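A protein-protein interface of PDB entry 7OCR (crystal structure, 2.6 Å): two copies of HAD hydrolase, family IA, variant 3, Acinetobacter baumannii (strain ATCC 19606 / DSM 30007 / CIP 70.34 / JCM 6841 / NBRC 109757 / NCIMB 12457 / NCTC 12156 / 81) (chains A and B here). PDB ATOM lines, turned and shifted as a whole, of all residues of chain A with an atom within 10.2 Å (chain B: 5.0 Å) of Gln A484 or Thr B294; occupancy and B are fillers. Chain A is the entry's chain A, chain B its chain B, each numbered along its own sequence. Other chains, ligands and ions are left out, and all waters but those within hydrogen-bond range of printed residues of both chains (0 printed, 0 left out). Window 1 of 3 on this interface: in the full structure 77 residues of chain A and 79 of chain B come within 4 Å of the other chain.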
ATOM      1  N   PHE A 292       1.659 -16.130  34.611  1.00  0.00           N
ATOM      2  CA  PHE A 292       1.044 -17.313  33.948  1.00  0.00           C
ATOM      3  C   PHE A 292      -0.077 -16.861  33.003  1.00  0.00           C
ATOM      4  O   PHE A 292      -0.329 -17.557  31.999  1.00  0.00           O
ATOM      5  CB  PHE A 292       0.507 -18.308  34.981  1.00  0.00           C
ATOM      6  CG  PHE A 292       1.440 -19.445  35.314  1.00  0.00           C
ATOM      7  CD1 PHE A 292       2.496 -19.266  36.195  1.00  0.00           C
ATOM      8  CD2 PHE A 292       1.257 -20.699  34.750  1.00  0.00           C
ATOM      9  CE1 PHE A 292       3.350 -20.316  36.500  1.00  0.00           C
ATOM     10  CE2 PHE A 292       2.113 -21.746  35.055  1.00  0.00           C
ATOM     11  CZ  PHE A 292       3.157 -21.553  35.929  1.00  0.00           C
ATOM     12  N   THR A 294      -3.141 -16.797  33.931  1.00  0.00           N
ATOM     13  CA  THR A 294      -4.204 -17.773  34.292  1.00  0.00           C
ATOM     14  C   THR A 294      -3.820 -18.484  35.595  1.00  0.00           C
ATOM     15  O   THR A 294      -2.620 -18.497  35.929  1.00  0.00           O
ATOM     16  CB  THR A 294      -4.430 -18.789  33.164  1.00  0.00           C
ATOM     17  OG1 THR A 294      -5.441 -19.704  33.587  1.00  0.00           O
ATOM     18  CG2 THR A 294      -3.181 -19.559  32.792  1.00  0.00           C
ATOM     19  N   SER A 296      -5.560 -22.097  38.218  1.00  0.00           N
ATOM     20  CA  SER A 296      -6.427 -23.305  38.214  1.00  0.00           C
ATOM     21  C   SER A 296      -6.994 -23.566  39.614  1.00  0.00           C
ATOM     22  O   SER A 296      -6.276 -23.316  40.605  1.00  0.00           O
ATOM     23  CB  SER A 296      -5.675 -24.497  37.689  1.00  0.00           C
ATOM     24  OG  SER A 296      -5.365 -24.330  36.314  1.00  0.00           O
ATOM     25  N   ASP A 305      -8.320 -30.275  37.765  1.00  0.00           N
ATOM     26  CA  ASP A 305      -7.787 -28.887  37.782  1.00  0.00           C
ATOM     27  C   ASP A 305      -8.573 -28.049  36.768  1.00  0.00           C
ATOM     28  O   ASP A 305      -8.473 -28.337  35.560  1.00  0.00           O
ATOM     29  CB  ASP A 305      -6.284 -28.866  37.490  1.00  0.00           C
ATOM     30  CG  ASP A 305      -5.441 -29.601  38.519  1.00  0.00           C
ATOM     31  OD1 ASP A 305      -5.995 -29.996  39.566  1.00  0.00           O
ATOM     32  OD2 ASP A 305      -4.231 -29.772  38.266  1.00  0.00           O
ATOM     33  N   ARG A 307      -9.024 -24.659  34.913  1.00  0.00           N
ATOM     34  CA  ARG A 307      -8.203 -23.494  34.481  1.00  0.00           C
ATOM     35  C   ARG A 307      -9.120 -22.292  34.221  1.00  0.00           C
ATOM     36  O   ARG A 307     -10.009 -22.403  33.354  1.00  0.00           O
ATOM     37  CB  ARG A 307      -7.373 -23.862  33.245  1.00  0.00           C
ATOM     38  CG  ARG A 307      -6.712 -22.680  32.550  1.00  0.00           C
ATOM     39  CD  ARG A 307      -5.239 -22.903  32.254  1.00  0.00           C
ATOM     40  NE  ARG A 307      -4.957 -24.182  31.614  1.00  0.00           N
ATOM     41  CZ  ARG A 307      -3.736 -24.664  31.385  1.00  0.00           C
ATOM     42  NH1 ARG A 307      -3.594 -25.841  30.799  1.00  0.00           N
ATOM     43  NH2 ARG A 307      -2.664 -23.974  31.739  1.00  0.00           N
ATOM     44  N   GLU A 309      -9.339 -18.671  32.709  1.00  0.00           N
ATOM     45  CA  GLU A 309      -8.679 -17.817  31.683  1.00  0.00           C
ATOM     46  C   GLU A 309      -9.141 -16.363  31.835  1.00  0.00           C
ATOM     47  O   GLU A 309     -10.157 -16.127  32.522  1.00  0.00           O
ATOM     48  CB  GLU A 309      -8.996 -18.327  30.276  1.00  0.00           C
ATOM     49  CG  GLU A 309      -8.285 -19.623  29.923  1.00  0.00           C
ATOM     50  CD  GLU A 309      -8.400 -20.033  28.464  1.00  0.00           C
ATOM     51  OE1 GLU A 309      -9.496 -19.869  27.886  1.00  0.00           O
ATOM     52  OE2 GLU A 309      -7.391 -20.510  27.907  1.00  0.00           O
ATOM     53  N   HIS A 440      12.732 -27.136  29.912  1.00  0.00           N
ATOM     54  CA  HIS A 440      11.995 -26.923  28.637  1.00  0.00           C
ATOM     55  C   HIS A 440      12.800 -26.010  27.702  1.00  0.00           C
ATOM     56  O   HIS A 440      12.765 -26.254  26.480  1.00  0.00           O
ATOM     57  CB  HIS A 440      10.588 -26.375  28.927  1.00  0.00           C
ATOM     58  CG  HIS A 440       9.856 -25.907  27.715  1.00  0.00           C
ATOM     59  ND1 HIS A 440       9.367 -26.780  26.763  1.00  0.00           N
ATOM     60  CD2 HIS A 440       9.529 -24.666  27.297  1.00  0.00           C
ATOM     61  CE1 HIS A 440       8.769 -26.095  25.810  1.00  0.00           C
ATOM     62  NE2 HIS A 440       8.856 -24.797  26.114  1.00  0.00           N
ATOM     63  N   MET A 473       6.751 -16.129  15.577  1.00  0.00           N
ATOM     64  CA  MET A 473       5.724 -16.828  16.398  1.00  0.00           C
ATOM     65  C   MET A 473       6.402 -17.867  17.301  1.00  0.00           C
ATOM     66  O   MET A 473       6.122 -17.859  18.516  1.00  0.00           O
ATOM     67  CB  MET A 473       4.686 -17.523  15.511  1.00  0.00           C
ATOM     68  CG  MET A 473       3.645 -16.574  14.949  1.00  0.00           C
ATOM     69  SD  MET A 473       2.609 -17.348  13.684  1.00  0.00           S
ATOM     70  CE  MET A 473       1.315 -16.119  13.525  1.00  0.00           C
ATOM     71  N   PHE A 477       6.230 -17.982  21.286  1.00  0.00           N
ATOM     72  CA  PHE A 477       5.237 -18.983  21.768  1.00  0.00           C
ATOM     73  C   PHE A 477       5.934 -20.196  22.398  1.00  0.00           C
ATOM     74  O   PHE A 477       5.425 -20.688  23.426  1.00  0.00           O
ATOM     75  CB  PHE A 477       4.321 -19.455  20.633  1.00  0.00           C
ATOM     76  CG  PHE A 477       3.407 -18.411  20.040  1.00  0.00           C
ATOM     77  CD1 PHE A 477       2.901 -17.370  20.806  1.00  0.00           C
ATOM     78  CD2 PHE A 477       3.021 -18.493  18.710  1.00  0.00           C
ATOM     79  CE1 PHE A 477       2.055 -16.424  20.249  1.00  0.00           C
ATOM     80  CE2 PHE A 477       2.172 -17.549  18.156  1.00  0.00           C
ATOM     81  CZ  PHE A 477       1.689 -16.516  18.926  1.00  0.00           C
ATOM     82  N   GLN A 478       7.041 -20.664  21.808  1.00  0.00           N
ATOM     83  CA  GLN A 478       7.697 -21.957  22.153  1.00  0.00           C
ATOM     84  C   GLN A 478       7.992 -22.026  23.651  1.00  0.00           C
ATOM     85  O   GLN A 478       7.719 -23.052  24.270  1.00  0.00           O
ATOM     86  CB  GLN A 478       8.961 -22.189  21.320  1.00  0.00           C
ATOM     87  CG  GLN A 478       9.457 -23.627  21.363  1.00  0.00           C
ATOM     88  CD  GLN A 478      10.665 -23.849  20.487  1.00  0.00           C
ATOM     89  OE1 GLN A 478      11.316 -22.908  20.037  1.00  0.00           O
ATOM     90  NE2 GLN A 478      10.978 -25.110  20.237  1.00  0.00           N
ATOM     91  N   PRO A 479       8.547 -20.968  24.292  1.00  0.00           N
ATOM     92  CA  PRO A 479       8.772 -20.984  25.741  1.00  0.00           C
ATOM     93  C   PRO A 479       7.506 -21.246  26.576  1.00  0.00           C
ATOM     94  O   PRO A 479       7.639 -21.783  27.661  1.00  0.00           O
ATOM     95  CB  PRO A 479       9.319 -19.579  26.040  1.00  0.00           C
ATOM     96  CG  PRO A 479       9.937 -19.137  24.733  1.00  0.00           C
ATOM     97  CD  PRO A 479       9.029 -19.722  23.672  1.00  0.00           C
ATOM     98  N   GLY A 480       6.331 -20.868  26.057  1.00  0.00           N
ATOM     99  CA  GLY A 480       5.025 -21.009  26.734  1.00  0.00           C
ATOM    100  C   GLY A 480       4.278 -22.275  26.337  1.00  0.00           C
ATOM    101  O   GLY A 480       3.092 -22.386  26.702  1.00  0.00           O
ATOM    102  N   HIS A 481       4.932 -23.201  25.624  1.00  0.00           N
ATOM    103  CA  HIS A 481       4.375 -24.525  25.229  1.00  0.00           C
ATOM    104  C   HIS A 481       4.151 -25.393  26.475  1.00  0.00           C
ATOM    105  O   HIS A 481       3.238 -26.239  26.444  1.00  0.00           O
ATOM    106  CB  HIS A 481       5.295 -25.222  24.215  1.00  0.00           C
ATOM    107  CG  HIS A 481       5.179 -24.682  22.830  1.00  0.00           C
ATOM    108  ND1 HIS A 481       4.568 -23.475  22.559  1.00  0.00           N
ATOM    109  CD2 HIS A 481       5.605 -25.168  21.643  1.00  0.00           C
ATOM    110  CE1 HIS A 481       4.608 -23.245  21.263  1.00  0.00           C
ATOM    111  NE2 HIS A 481       5.242 -24.268  20.678  1.00  0.00           N
ATOM    112  N   ILE A 482       4.958 -25.184  27.521  1.00  0.00           N
ATOM    113  CA  ILE A 482       4.905 -25.936  28.811  1.00  0.00           C
ATOM    114  C   ILE A 482       3.544 -25.703  29.486  1.00  0.00           C
ATOM    115  O   ILE A 482       3.081 -26.620  30.194  1.00  0.00           O
ATOM    116  CB  ILE A 482       6.090 -25.541  29.720  1.00  0.00           C
ATOM    117  CG1 ILE A 482       6.334 -26.567  30.830  1.00  0.00           C
ATOM    118  CG2 ILE A 482       5.914 -24.137  30.282  1.00  0.00           C
ATOM    119  CD1 ILE A 482       6.954 -27.861  30.352  1.00  0.00           C
ATOM    120  N   LEU A 483       2.920 -24.540  29.258  1.00  0.00           N
ATOM    121  CA  LEU A 483       1.627 -24.133  29.879  1.00  0.00           C
ATOM    122  C   LEU A 483       0.484 -25.052  29.421  1.00  0.00           C
ATOM    123  O   LEU A 483      -0.557 -25.058  30.107  1.00  0.00           O
ATOM    124  CB  LEU A 483       1.319 -22.673  29.522  1.00  0.00           C
ATOM    125  CG  LEU A 483       2.289 -21.629  30.075  1.00  0.00           C
ATOM    126  CD1 LEU A 483       1.861 -20.228  29.668  1.00  0.00           C
ATOM    127  CD2 LEU A 483       2.403 -21.731  31.589  1.00  0.00           C
ATOM    128  N   GLN A 484       0.657 -25.778  28.308  1.00  0.00           N
ATOM    129  CA  GLN A 484      -0.331 -26.758  27.774  1.00  0.00           C
ATOM    130  C   GLN A 484      -0.760 -27.716  28.894  1.00  0.00           C
ATOM    131  O   GLN A 484      -1.978 -27.812  29.151  1.00  0.00           O
ATOM    132  CB  GLN A 484       0.252 -27.541  26.594  1.00  0.00           C
ATOM    133  CG  GLN A 484       0.316 -26.743  25.298  1.00  0.00           C
ATOM    134  CD  GLN A 484       0.983 -27.509  24.180  1.00  0.00           C
ATOM    135  OE1 GLN A 484       0.706 -28.687  23.953  1.00  0.00           O
ATOM    136  NE2 GLN A 484       1.868 -26.840  23.460  1.00  0.00           N
ATOM    137  N   SER A 485       0.208 -28.388  29.528  1.00  0.00           N
ATOM    138  CA  SER A 485       0.003 -29.349  30.645  1.00  0.00           C
ATOM    139  C   SER A 485       0.777 -28.877  31.884  1.00  0.00           C
ATOM    140  O   SER A 485       1.582 -29.665  32.422  1.00  0.00           O
ATOM    141  CB  SER A 485       0.402 -30.747  30.235  1.00  0.00           C
ATOM    142  OG  SER A 485       1.794 -30.820  29.962  1.00  0.00           O
ATOM    143  N   MET A 486       0.540 -27.630  32.305  1.00  0.00           N
ATOM    144  CA  MET A 486       1.114 -27.016  33.534  1.00  0.00           C
ATOM    145  C   MET A 486       0.117 -25.988  34.082  1.00  0.00           C
ATOM    146  O   MET A 486      -0.184 -25.017  33.361  1.00  0.00           O
ATOM    147  CB  MET A 486       2.450 -26.325  33.240  1.00  0.00           C
ATOM    148  CG  MET A 486       3.091 -25.690  34.464  1.00  0.00           C
ATOM    149  SD  MET A 486       4.789 -25.138  34.164  1.00  0.00           S
ATOM    150  CE  MET A 486       5.644 -26.713  34.141  1.00  0.00           C
ATOM    151  N   ASP A 487      -0.367 -26.205  35.310  1.00  0.00           N
ATOM    152  CA  ASP A 487      -1.411 -25.379  35.972  1.00  0.00           C
ATOM    153  C   ASP A 487      -0.817 -24.698  37.210  1.00  0.00           C
ATOM    154  O   ASP A 487      -0.050 -25.360  37.936  1.00  0.00           O
ATOM    155  CB  ASP A 487      -2.620 -26.234  36.357  1.00  0.00           C
ATOM    156  CG  ASP A 487      -3.333 -26.854  35.167  1.00  0.00           C
ATOM    157  OD1 ASP A 487      -2.696 -27.660  34.460  1.00  0.00           O
ATOM    158  OD2 ASP A 487      -4.515 -26.519  34.952  1.00  0.00           O
ATOM    159  N   LEU A 488      -1.167 -23.427  37.434  1.00  0.00           N
ATOM    160  CA  LEU A 488      -0.846 -22.667  38.672  1.00  0.00           C
ATOM    161  C   LEU A 488      -1.998 -22.850  39.669  1.00  0.00           C
ATOM    162  O   LEU A 488      -2.954 -22.050  39.629  1.00  0.00           O
ATOM    163  CB  LEU A 488      -0.627 -21.191  38.320  1.00  0.00           C
ATOM    164  CG  LEU A 488      -0.172 -20.296  39.471  1.00  0.00           C
ATOM    165  CD1 LEU A 488       1.211 -20.700  39.962  1.00  0.00           C
ATOM    166  CD2 LEU A 488      -0.183 -18.832  39.056  1.00  0.00           C
ATOM    167  N   VAL B 289       2.442 -25.746  13.247  1.00  0.00           N
ATOM    168  CA  VAL B 289       1.968 -26.523  14.434  1.00  0.00           C
ATOM    169  C   VAL B 289       3.043 -26.465  15.526  1.00  0.00           C
ATOM    170  O   VAL B 289       2.691 -26.151  16.679  1.00  0.00           O
ATOM    171  CB  VAL B 289       1.623 -27.980  14.067  1.00  0.00           C
ATOM    172  CG1 VAL B 289       1.335 -28.824  15.302  1.00  0.00           C
ATOM    173  CG2 VAL B 289       0.460 -28.063  13.089  1.00  0.00           C
ATOM    174  N   PHE B 292       3.218 -22.914  17.103  1.00  0.00           N
ATOM    175  CA  PHE B 292       2.038 -22.658  17.975  1.00  0.00           C
ATOM    176  C   PHE B 292       2.064 -23.600  19.186  1.00  0.00           C
ATOM    177  O   PHE B 292       1.669 -23.165  20.285  1.00  0.00           O
ATOM    178  CB  PHE B 292       0.728 -22.814  17.195  1.00  0.00           C
ATOM    179  CG  PHE B 292       0.183 -21.532  16.618  1.00  0.00           C
ATOM    180  CD1 PHE B 292       0.664 -21.029  15.418  1.00  0.00           C
ATOM    181  CD2 PHE B 292      -0.812 -20.825  17.277  1.00  0.00           C
ATOM    182  CE1 PHE B 292       0.162 -19.849  14.891  1.00  0.00           C
ATOM    183  CE2 PHE B 292      -1.313 -19.645  16.748  1.00  0.00           C
ATOM    184  CZ  PHE B 292      -0.826 -19.159  15.556  1.00  0.00           C
ATOM    185  N   GLY B 293       2.497 -24.848  18.981  1.00  0.00           N
ATOM    186  CA  GLY B 293       2.532 -25.904  20.013  1.00  0.00           C
ATOM    187  C   GLY B 293       1.277 -26.759  19.988  1.00  0.00           C
ATOM    188  O   GLY B 293       1.305 -27.865  20.563  1.00  0.00           O
ATOM    189  N   THR B 294       0.210 -26.258  19.355  1.00  0.00           N
ATOM    190  CA  THR B 294      -1.093 -26.953  19.178  1.00  0.00           C
ATOM    191  C   THR B 294      -1.681 -26.596  17.808  1.00  0.00           C
ATOM    192  O   THR B 294      -1.145 -25.681  17.149  1.00  0.00           O
ATOM    193  CB  THR B 294      -2.079 -26.577  20.292  1.00  0.00           C
ATOM    194  OG1 THR B 294      -2.365 -25.181  20.182  1.00  0.00           O
ATOM    195  CG2 THR B 294      -1.553 -26.880  21.678  1.00  0.00           C
ATOM    196  N   TYR B 295      -2.737 -27.307  17.406  1.00  0.00           N
ATOM    197  CA  TYR B 295      -3.640 -26.953  16.281  1.00  0.00           C
ATOM    198  C   TYR B 295      -5.068 -27.341  16.677  1.00  0.00           C
ATOM    199  O   TYR B 295      -5.223 -28.217  17.551  1.00  0.00           O
ATOM    200  CB  TYR B 295      -3.197 -27.633  14.983  1.00  0.00           C
ATOM    201  CG  TYR B 295      -3.547 -29.096  14.892  1.00  0.00           C
ATOM    202  CD1 TYR B 295      -4.787 -29.506  14.426  1.00  0.00           C
ATOM    203  CD2 TYR B 295      -2.645 -30.073  15.279  1.00  0.00           C
ATOM    204  CE1 TYR B 295      -5.121 -30.849  14.348  1.00  0.00           C
ATOM    205  CE2 TYR B 295      -2.962 -31.419  15.204  1.00  0.00           C
ATOM    206  CZ  TYR B 295      -4.203 -31.808  14.737  1.00  0.00           C
ATOM    207  OH  TYR B 295      -4.515 -33.134  14.662  1.00  0.00           O
ATOM    208  N   SER B 296      -6.067 -26.709  16.056  1.00  0.00           N
ATOM    209  CA  SER B 296      -7.509 -26.913  16.348  1.00  0.00           C
ATOM    210  C   SER B 296      -8.215 -27.531  15.135  1.00  0.00           C
ATOM    211  O   SER B 296      -7.865 -27.166  13.995  1.00  0.00           O
ATOM    212  CB  SER B 296      -8.160 -25.623  16.769  1.00  0.00           C
ATOM    213  OG  SER B 296      -7.822 -25.303  18.109  1.00  0.00           O
ATOM    214  N   ARG B 307      -9.067 -28.009  20.313  1.00  0.00           N
ATOM    215  CA  ARG B 307      -7.594 -27.844  20.447  1.00  0.00           C
ATOM    216  C   ARG B 307      -6.950 -29.218  20.679  1.00  0.00           C
ATOM    217  O   ARG B 307      -7.248 -29.842  21.717  1.00  0.00           O
ATOM    218  CB  ARG B 307      -7.271 -26.867  21.584  1.00  0.00           C
ATOM    219  CG  ARG B 307      -5.783 -26.682  21.848  1.00  0.00           C
ATOM    220  CD  ARG B 307      -5.491 -25.627  22.899  1.00  0.00           C
ATOM    221  NE  ARG B 307      -5.372 -24.288  22.329  1.00  0.00           N
ATOM    222  CZ  ARG B 307      -6.346 -23.380  22.266  1.00  0.00           C
ATOM    223  NH1 ARG B 307      -6.100 -22.199  21.719  1.00  0.00           N
ATOM    224  NH2 ARG B 307      -7.553 -23.637  22.743  1.00  0.00           N
ATOM    225  N   ILE B 308      -6.108 -29.661  19.739  1.00  0.00           N
ATOM    226  CA  ILE B 308      -5.286 -30.907  19.835  1.00  0.00           C
ATOM    227  C   ILE B 308      -3.879 -30.513  20.300  1.00  0.00           C
ATOM    228  O   ILE B 308      -3.238 -29.706  19.598  1.00  0.00           O
ATOM    229  CB  ILE B 308      -5.251 -31.655  18.485  1.00  0.00           C
ATOM    230  CG1 ILE B 308      -6.649 -31.853  17.893  1.00  0.00           C
ATOM    231  CG2 ILE B 308      -4.503 -32.972  18.619  1.00  0.00           C
ATOM    232  CD1 ILE B 308      -7.599 -32.628  18.779  1.00  0.00           C
ATOM    233  N   GLU B 309      -3.419 -31.069  21.426  1.00  0.00           N
ATOM    234  CA  GLU B 309      -2.130 -30.702  22.074  1.00  0.00           C
ATOM    235  C   GLU B 309      -1.262 -31.955  22.254  1.00  0.00           C
ATOM    236  O   GLU B 309      -1.782 -33.073  22.063  1.00  0.00           O
ATOM    237  CB  GLU B 309      -2.374 -29.960  23.395  1.00  0.00           C
ATOM    238  CG  GLU B 309      -3.436 -30.580  24.289  1.00  0.00           C
ATOM    239  CD  GLU B 309      -3.741 -29.785  25.549  1.00  0.00           C
ATOM    240  OE1 GLU B 309      -3.581 -28.548  25.523  1.00  0.00           O
ATOM    241  OE2 GLU B 309      -4.140 -30.404  26.556  1.00  0.00           O
ATOM    242  N   ASN B 310       0.018 -31.751  22.590  1.00  0.00           N
ATOM    243  CA  ASN B 310       1.069 -32.800  22.697  1.00  0.00           C
ATOM    244  C   ASN B 310       1.362 -33.365  21.302  1.00  0.00           C
ATOM    245  O   ASN B 310       1.584 -34.588  21.192  1.00  0.00           O
ATOM    246  CB  ASN B 310       0.682 -33.905  23.684  1.00  0.00           C
ATOM    247  CG  ASN B 310       0.356 -33.379  25.065  1.00  0.00           C
ATOM    248  OD1 ASN B 310       1.044 -32.501  25.579  1.00  0.00           O
ATOM    249  ND2 ASN B 310      -0.691 -33.913  25.673  1.00  0.00           N
ATOM    250  N   LEU B 488      -4.981 -22.249  16.040  1.00  0.00           N
ATOM    251  CA  LEU B 488      -4.448 -22.561  14.684  1.00  0.00           C
ATOM    252  C   LEU B 488      -5.395 -23.556  14.000  1.00  0.00           C
ATOM    253  O   LEU B 488      -5.318 -24.759  14.315  1.00  0.00           O
ATOM    254  CB  LEU B 488      -3.030 -23.128  14.815  1.00  0.00           C
ATOM    255  CG  LEU B 488      -2.321 -23.451  13.500  1.00  0.00           C
ATOM    256  CD1 LEU B 488      -2.012 -22.182  12.722  1.00  0.00           C
ATOM    257  CD2 LEU B 488      -1.046 -24.242  13.751  1.00  0.00           C
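Among the printed residues, pairs that only touch across the chains: His A481 with Phe B292, Gln A484 with Glu B309, Gln A484 with Thr B294 and Met A473 with Phe B292.
Of the 20 printed residues of chain A, 3 touch a printed residue of chain B.
Hydrophobic or aromatic side chains of chain A within 4 Å of the printed part of chain B: Met A473 and His A481.
Hydrophobic or aromatic side chains of chain B that line the printed part of chain A: Phe B292.
Among the printed residues, no Asp or Glu carboxylate lies within 4 Å of a Lys or Arg side-chain nitrogen of the other chain.
NE2 of His A481 sits close to N of Gly B293 (3.3 Å).
The backbone carbonyl oxygen of Gly B293 is in hydrogen-bond range of the side-chain amide nitrogen of Gln A484 (3.1 Å).
OE1 of Gln A484 sits at hydrogen-bond distance from N of Asn B310 (3.4 Å).
Positions printed for both chains: 292, 294, 296, 307, 309 and 488.
Of the 7 pairs that touch across the chains among the printed residues, none has its exchanged pair printed and touching as well.
The guanidinium group of Arg A307 is in hydrogen-bond range of the backbone carbonyl oxygen of Gln A484 (3.0 Å).
O of Phe A477 is in hydrogen-bond range of ND1 of His A481.
O of His A481 sits close to NE2 of Gln A484, 3.3 Å away.
Arg A307 touches none of the printed residues of chain B.
Of the printed residues of chain B, Met A473 touches Phe B292.
Printed residues of chain B within 4 Å of His A481: Phe B292 and Gly B293.
Gln A484 touches just these residues of chain B: Gly B293, Thr B294, Glu B309 and Asn B310.
Val B289 touches none of the printed residues of chain A.
Printed residues of chain A within 4 Å of Phe B292: Met A473 and His A481.
Of chain A, only His A481 (3.2 Å) and Gln A484 (3.1 Å) come within 4 Å of Gly B293.
Thr B294 touches just one residue of chain A: Gln A484 (3.6 Å).
Arg B307 touches none of the printed residues of chain A.
Of chain A, only Gln A484 (3.4 Å) comes within 4 Å of Glu B309.
Printed residues of chain A within 4 Å of Asn B310: Gln A484.
Leu B488 touches none of the printed residues of chain A.
The nearest residue of chain A that does not touch Thr B294 is His A481 (5.6 Å).
The nearest printed residue of chain B that does not touch Met A473 is Leu B488 (6.8 Å).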
